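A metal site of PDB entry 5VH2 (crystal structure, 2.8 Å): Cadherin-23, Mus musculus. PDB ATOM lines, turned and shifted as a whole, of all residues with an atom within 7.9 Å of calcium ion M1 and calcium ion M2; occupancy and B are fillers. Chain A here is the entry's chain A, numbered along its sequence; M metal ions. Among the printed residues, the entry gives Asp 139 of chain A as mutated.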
ATOM      1  N   GLU A  20      -6.118 -28.201  21.514  1.00  0.00           N
ATOM      2  CA  GLU A  20      -6.626 -28.927  22.698  1.00  0.00           C
ATOM      3  C   GLU A  20      -6.867 -30.406  22.417  1.00  0.00           C
ATOM      4  O   GLU A  20      -6.743 -31.223  23.336  1.00  0.00           O
ATOM      5  CB  GLU A  20      -7.893 -28.276  23.293  1.00  0.00           C
ATOM      6  CG  GLU A  20      -9.101 -28.362  22.409  1.00  0.00           C
ATOM      7  CD  GLU A  20     -10.417 -28.068  23.106  1.00  0.00           C
ATOM      8  OE1 GLU A  20     -10.649 -28.512  24.265  1.00  0.00           O
ATOM      9  OE2 GLU A  20     -11.268 -27.411  22.452  1.00  0.00           O
ATOM     10  N   THR A  21      -7.164 -30.744  21.162  1.00  0.00           N
ATOM     11  CA  THR A  21      -7.340 -32.153  20.755  1.00  0.00           C
ATOM     12  C   THR A  21      -6.036 -32.833  20.366  1.00  0.00           C
ATOM     13  O   THR A  21      -6.056 -33.931  19.803  1.00  0.00           O
ATOM     14  CB  THR A  21      -8.345 -32.316  19.576  1.00  0.00           C
ATOM     15  OG1 THR A  21      -7.831 -31.679  18.395  1.00  0.00           O
ATOM     16  CG2 THR A  21      -9.716 -31.758  19.928  1.00  0.00           C
ATOM     17  N   LEU A  71      -6.019 -33.090  26.686  1.00  0.00           N
ATOM     18  CA  LEU A  71      -6.213 -31.709  27.079  1.00  0.00           C
ATOM     19  C   LEU A  71      -7.646 -31.316  26.820  1.00  0.00           C
ATOM     20  O   LEU A  71      -8.380 -32.061  26.162  1.00  0.00           O
ATOM     21  CB  LEU A  71      -5.249 -30.778  26.335  1.00  0.00           C
ATOM     22  CG  LEU A  71      -3.771 -31.107  26.509  1.00  0.00           C
ATOM     23  CD1 LEU A  71      -2.969 -30.421  25.420  1.00  0.00           C
ATOM     24  CD2 LEU A  71      -3.318 -30.660  27.891  1.00  0.00           C
ATOM     25  N   ASP A  72      -8.053 -30.214  27.468  1.00  0.00           N
ATOM     26  CA  ASP A  72      -9.390 -29.692  27.300  1.00  0.00           C
ATOM     27  C   ASP A  72      -9.433 -28.175  27.529  1.00  0.00           C
ATOM     28  O   ASP A  72      -9.246 -27.680  28.667  1.00  0.00           O
ATOM     29  CB  ASP A  72     -10.319 -30.445  28.244  1.00  0.00           C
ATOM     30  CG  ASP A  72     -11.787 -30.145  28.007  1.00  0.00           C
ATOM     31  OD1 ASP A  72     -12.134 -29.509  26.964  1.00  0.00           O
ATOM     32  OD2 ASP A  72     -12.581 -30.589  28.873  1.00  0.00           O
ATOM     33  N   TYR A  73      -9.695 -27.428  26.450  1.00  0.00           N
ATOM     34  CA  TYR A  73      -9.896 -25.992  26.522  1.00  0.00           C
ATOM     35  C   TYR A  73     -10.986 -25.631  27.529  1.00  0.00           C
ATOM     36  O   TYR A  73     -10.834 -24.715  28.350  1.00  0.00           O
ATOM     37  CB  TYR A  73     -10.274 -25.444  25.169  1.00  0.00           C
ATOM     38  CG  TYR A  73     -10.371 -23.950  25.115  1.00  0.00           C
ATOM     39  CD1 TYR A  73      -9.232 -23.168  24.891  1.00  0.00           C
ATOM     40  CD2 TYR A  73     -11.572 -23.296  25.258  1.00  0.00           C
ATOM     41  CE1 TYR A  73      -9.291 -21.793  24.836  1.00  0.00           C
ATOM     42  CE2 TYR A  73     -11.645 -21.894  25.207  1.00  0.00           C
ATOM     43  CZ  TYR A  73     -10.495 -21.155  24.997  1.00  0.00           C
ATOM     44  OH  TYR A  73     -10.514 -19.779  24.937  1.00  0.00           O
ATOM     45  N   GLU A  74     -12.067 -26.388  27.478  1.00  0.00           N
ATOM     46  CA  GLU A  74     -13.238 -26.158  28.322  1.00  0.00           C
ATOM     47  C   GLU A  74     -13.032 -26.520  29.785  1.00  0.00           C
ATOM     48  O   GLU A  74     -13.859 -26.153  30.598  1.00  0.00           O
ATOM     49  CB  GLU A  74     -14.444 -26.916  27.771  1.00  0.00           C
ATOM     50  CG  GLU A  74     -15.130 -26.293  26.540  1.00  0.00           C
ATOM     51  CD  GLU A  74     -14.339 -26.417  25.233  1.00  0.00           C
ATOM     52  OE1 GLU A  74     -14.463 -25.500  24.394  1.00  0.00           O
ATOM     53  OE2 GLU A  74     -13.604 -27.409  25.027  1.00  0.00           O
ATOM     54  N   THR A  75     -11.971 -27.240  30.148  1.00  0.00           N
ATOM     55  CA  THR A  75     -11.611 -27.464  31.569  1.00  0.00           C
ATOM     56  C   THR A  75     -10.446 -26.586  32.034  1.00  0.00           C
ATOM     57  O   THR A  75     -10.427 -26.174  33.189  1.00  0.00           O
ATOM     58  CB  THR A  75     -11.224 -28.917  31.830  1.00  0.00           C
ATOM     59  OG1 THR A  75     -12.303 -29.777  31.460  1.00  0.00           O
ATOM     60  CG2 THR A  75     -10.860 -29.131  33.333  1.00  0.00           C
ATOM     61  N   LEU A 104      -5.613 -23.923  22.135  1.00  0.00           N
ATOM     62  CA  LEU A 104      -6.446 -23.453  21.043  1.00  0.00           C
ATOM     63  C   LEU A 104      -7.783 -24.174  21.159  1.00  0.00           C
ATOM     64  O   LEU A 104      -7.839 -25.394  21.090  1.00  0.00           O
ATOM     65  CB  LEU A 104      -5.756 -23.743  19.710  1.00  0.00           C
ATOM     66  CG  LEU A 104      -6.556 -23.700  18.398  1.00  0.00           C
ATOM     67  CD1 LEU A 104      -7.141 -22.331  18.187  1.00  0.00           C
ATOM     68  CD2 LEU A 104      -5.634 -24.046  17.247  1.00  0.00           C
ATOM     69  N   ASN A 105      -8.853 -23.431  21.402  1.00  0.00           N
ATOM     70  CA  ASN A 105     -10.202 -24.004  21.368  1.00  0.00           C
ATOM     71  C   ASN A 105     -10.489 -24.566  19.978  1.00  0.00           C
ATOM     72  O   ASN A 105     -10.320 -23.898  18.979  1.00  0.00           O
ATOM     73  CB  ASN A 105     -11.223 -22.944  21.732  1.00  0.00           C
ATOM     74  CG  ASN A 105     -12.620 -23.535  21.901  1.00  0.00           C
ATOM     75  OD1 ASN A 105     -12.812 -24.743  22.117  1.00  0.00           O
ATOM     76  ND2 ASN A 105     -13.622 -22.657  21.800  1.00  0.00           N
ATOM     77  N   GLU A 106     -10.856 -25.836  19.945  1.00  0.00           N
ATOM     78  CA  GLU A 106     -11.297 -26.466  18.719  1.00  0.00           C
ATOM     79  C   GLU A 106     -12.684 -27.014  18.935  1.00  0.00           C
ATOM     80  O   GLU A 106     -13.133 -27.156  20.074  1.00  0.00           O
ATOM     81  CB  GLU A 106     -10.388 -27.628  18.385  1.00  0.00           C
ATOM     82  CG  GLU A 106      -8.907 -27.317  18.291  1.00  0.00           C
ATOM     83  CD  GLU A 106      -8.153 -28.475  17.665  1.00  0.00           C
ATOM     84  OE1 GLU A 106      -8.221 -28.619  16.414  1.00  0.00           O
ATOM     85  OE2 GLU A 106      -7.544 -29.272  18.413  1.00  0.00           O
ATOM     86  N   LEU A 107     -13.361 -27.323  17.837  1.00  0.00           N
ATOM     87  CA  LEU A 107     -14.720 -27.824  17.883  1.00  0.00           C
ATOM     88  C   LEU A 107     -14.731 -29.307  18.253  1.00  0.00           C
ATOM     89  O   LEU A 107     -14.718 -30.180  17.378  1.00  0.00           O
ATOM     90  CB  LEU A 107     -15.367 -27.597  16.533  1.00  0.00           C
ATOM     91  CG  LEU A 107     -16.898 -27.691  16.490  1.00  0.00           C
ATOM     92  CD1 LEU A 107     -17.610 -26.483  17.099  1.00  0.00           C
ATOM     93  CD2 LEU A 107     -17.294 -27.849  15.028  1.00  0.00           C
ATOM     94  N   ASP A 108     -14.804 -29.572  19.546  1.00  0.00           N
ATOM     95  CA  ASP A 108     -14.798 -30.930  20.103  1.00  0.00           C
ATOM     96  C   ASP A 108     -15.887 -31.180  21.167  1.00  0.00           C
ATOM     97  O   ASP A 108     -15.793 -32.123  21.933  1.00  0.00           O
ATOM     98  CB  ASP A 108     -13.419 -31.210  20.716  1.00  0.00           C
ATOM     99  CG  ASP A 108     -13.117 -30.343  21.941  1.00  0.00           C
ATOM    100  OD1 ASP A 108     -13.702 -29.248  22.091  1.00  0.00           O
ATOM    101  OD2 ASP A 108     -12.278 -30.737  22.759  1.00  0.00           O
ATOM    102  N   GLU A 109     -16.902 -30.326  21.219  1.00  0.00           N
ATOM    103  CA  GLU A 109     -17.907 -30.424  22.278  1.00  0.00           C
ATOM    104  C   GLU A 109     -19.310 -30.372  21.694  1.00  0.00           C
ATOM    105  O   GLU A 109     -19.477 -29.988  20.550  1.00  0.00           O
ATOM    106  CB  GLU A 109     -17.759 -29.310  23.322  1.00  0.00           C
ATOM    107  CG  GLU A 109     -16.419 -29.233  24.024  1.00  0.00           C
ATOM    108  CD  GLU A 109     -16.184 -30.397  24.961  1.00  0.00           C
ATOM    109  OE1 GLU A 109     -15.068 -30.470  25.495  1.00  0.00           O
ATOM    110  OE2 GLU A 109     -17.099 -31.211  25.154  1.00  0.00           O
ATOM    111  N   ALA A 110     -20.299 -30.709  22.528  1.00  0.00           N
ATOM    112  CA  ALA A 110     -21.681 -30.825  22.105  1.00  0.00           C
ATOM    113  C   ALA A 110     -22.373 -29.461  22.111  1.00  0.00           C
ATOM    114  O   ALA A 110     -21.731 -28.438  21.795  1.00  0.00           O
ATOM    115  CB  ALA A 110     -22.415 -31.840  22.989  1.00  0.00           C
ATOM    116  N   ASP A 139     -23.809 -23.592  20.897  1.00  0.00           N
ATOM    117  CA  ASP A 139     -22.598 -24.386  20.790  1.00  0.00           C
ATOM    118  C   ASP A 139     -21.745 -24.206  22.051  1.00  0.00           C
ATOM    119  O   ASP A 139     -21.244 -23.105  22.337  1.00  0.00           O
ATOM    120  CB  ASP A 139     -21.803 -23.922  19.566  1.00  0.00           C
ATOM    121  CG  ASP A 139     -20.483 -24.602  19.416  1.00  0.00           C
ATOM    122  OD1 ASP A 139     -20.366 -25.756  19.885  1.00  0.00           O
ATOM    123  OD2 ASP A 139     -19.581 -23.985  18.811  1.00  0.00           O
ATOM    124  N   ILE A 140     -21.576 -25.301  22.796  1.00  0.00           N
ATOM    125  CA  ILE A 140     -20.686 -25.312  23.946  1.00  0.00           C
ATOM    126  C   ILE A 140     -19.321 -24.742  23.604  1.00  0.00           C
ATOM    127  O   ILE A 140     -18.783 -23.960  24.360  1.00  0.00           O
ATOM    128  CB  ILE A 140     -20.550 -26.733  24.547  1.00  0.00           C
ATOM    129  CG1 ILE A 140     -21.864 -27.141  25.232  1.00  0.00           C
ATOM    130  CG2 ILE A 140     -19.388 -26.796  25.535  1.00  0.00           C
ATOM    131  CD1 ILE A 140     -21.977 -28.622  25.537  1.00  0.00           C
ATOM    132  N   ASP A 141     -18.776 -25.120  22.446  1.00  0.00           N
ATOM    133  CA  ASP A 141     -17.451 -24.659  22.005  1.00  0.00           C
ATOM    134  C   ASP A 141     -17.333 -23.164  21.768  1.00  0.00           C
ATOM    135  O   ASP A 141     -16.215 -22.627  21.752  1.00  0.00           O
ATOM    136  CB  ASP A 141     -17.020 -25.364  20.712  1.00  0.00           C
ATOM    137  CG  ASP A 141     -16.743 -26.828  20.892  1.00  0.00           C
ATOM    138  OD1 ASP A 141     -15.666 -27.202  21.432  1.00  0.00           O
ATOM    139  OD2 ASP A 141     -17.620 -27.626  20.475  1.00  0.00           O
ATOM    140  N   ASN A 142     -18.486 -22.498  21.547  1.00  0.00           N
ATOM    141  CA  ASN A 142     -18.542 -21.057  21.274  1.00  0.00           C
ATOM    142  C   ASN A 142     -17.791 -20.677  20.000  1.00  0.00           C
ATOM    143  O   ASN A 142     -17.234 -19.590  19.896  1.00  0.00           O
ATOM    144  CB  ASN A 142     -18.059 -20.276  22.498  1.00  0.00           C
ATOM    145  CG  ASN A 142     -18.988 -20.436  23.677  1.00  0.00           C
ATOM    146  OD1 ASN A 142     -20.181 -20.652  23.490  1.00  0.00           O
ATOM    147  ND2 ASN A 142     -18.462 -20.323  24.891  1.00  0.00           N
ATOM    148  N   LEU A 143     -17.809 -21.582  19.016  1.00  0.00           N
ATOM    149  CA  LEU A 143     -17.220 -21.342  17.703  1.00  0.00           C
ATOM    150  C   LEU A 143     -18.288 -21.197  16.615  1.00  0.00           C
ATOM    151  O   LEU A 143     -18.247 -20.249  15.850  1.00  0.00           O
ATOM    152  CB  LEU A 143     -16.291 -22.476  17.347  1.00  0.00           C
ATOM    153  CG  LEU A 143     -15.076 -22.729  18.275  1.00  0.00           C
ATOM    154  CD1 LEU A 143     -14.490 -24.077  17.991  1.00  0.00           C
ATOM    155  CD2 LEU A 143     -13.997 -21.685  18.076  1.00  0.00           C
ATOM    156  N   LYS A 197     -19.718 -34.624  17.752  1.00  0.00           N
ATOM    157  CA  LYS A 197     -20.414 -35.342  18.833  1.00  0.00           C
ATOM    158  C   LYS A 197     -21.642 -36.150  18.422  1.00  0.00           C
ATOM    159  O   LYS A 197     -22.265 -35.846  17.416  1.00  0.00           O
ATOM    160  CB  LYS A 197     -20.769 -34.398  19.993  1.00  0.00           C
ATOM    161  CG  LYS A 197     -19.521 -33.934  20.765  1.00  0.00           C
ATOM    162  CD  LYS A 197     -18.795 -35.033  21.557  1.00  0.00           C
ATOM    163  CE  LYS A 197     -18.210 -34.439  22.848  1.00  0.00           C
ATOM    164  NZ  LYS A 197     -17.143 -35.282  23.460  1.00  0.00           N
HETATM  165 CA    CA M   1     -13.423 -26.805  22.334  1.00  0.00          CA
HETATM  166 CA    CA M   2     -13.212 -29.315  24.691  1.00  0.00          CA
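Calcium ion M1 is bound by the side-chain amide oxygen (OD1) of Asn 105, the side-chain carboxylate (OE2) of Glu 20, the backbone carbonyl oxygen (O) of Glu 106, the side-chain carboxylate (OD1) of Asp 141, the side-chain carboxylate (OD1) of Asp 108, the side-chain carboxylate (OE1) of Glu 74 and the side-chain carboxylate (OE2) of Glu 74.
Calcium ion M1 has seven donor atoms within binding distance.
The nearest printed residue that does not touch calcium ion M2 is Tyr 73 (4.4 Å).
Calcium ion M2 is bound by OE2 of Glu 74 (2.0 Å).
Calcium ion M2 is bound by the side-chain carboxylate (OE1) of Glu 109.
OD1 of Asp 72 binds calcium ion M2, at 2.5 Å.
The side-chain carboxylate (OD2) of Asp 108 binds calcium ion M2 (2.6 Å).
OD1 of Asp 108 is bound to calcium ion M2, at 2.6 Å.
OE1 of Glu 20 is bound to calcium ion M2.
Calcium ion M2 has six donor atoms within binding distance.
OD2 of Asp 141 is in hydrogen-bond range of N of Glu 109, at 2.9 Å.
OD2 of Asp 72 lies within hydrogen-bond range of OG1 of Thr 75.
N of Tyr 73 sits close to OE1 of Glu 20.
O of Leu 104 is in hydrogen-bond range of N of Glu 20.
The side-chain carboxylate of Asp 139 lies within hydrogen-bond range of the backbone NH of Asp 141, 3.1 Å away.
OE2 of Glu 106 is in hydrogen-bond range of OG1 of Thr 21, at 2.4 Å.
The nearest printed residue that does not touch calcium ion M1 is Glu 109 (4.2 Å).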
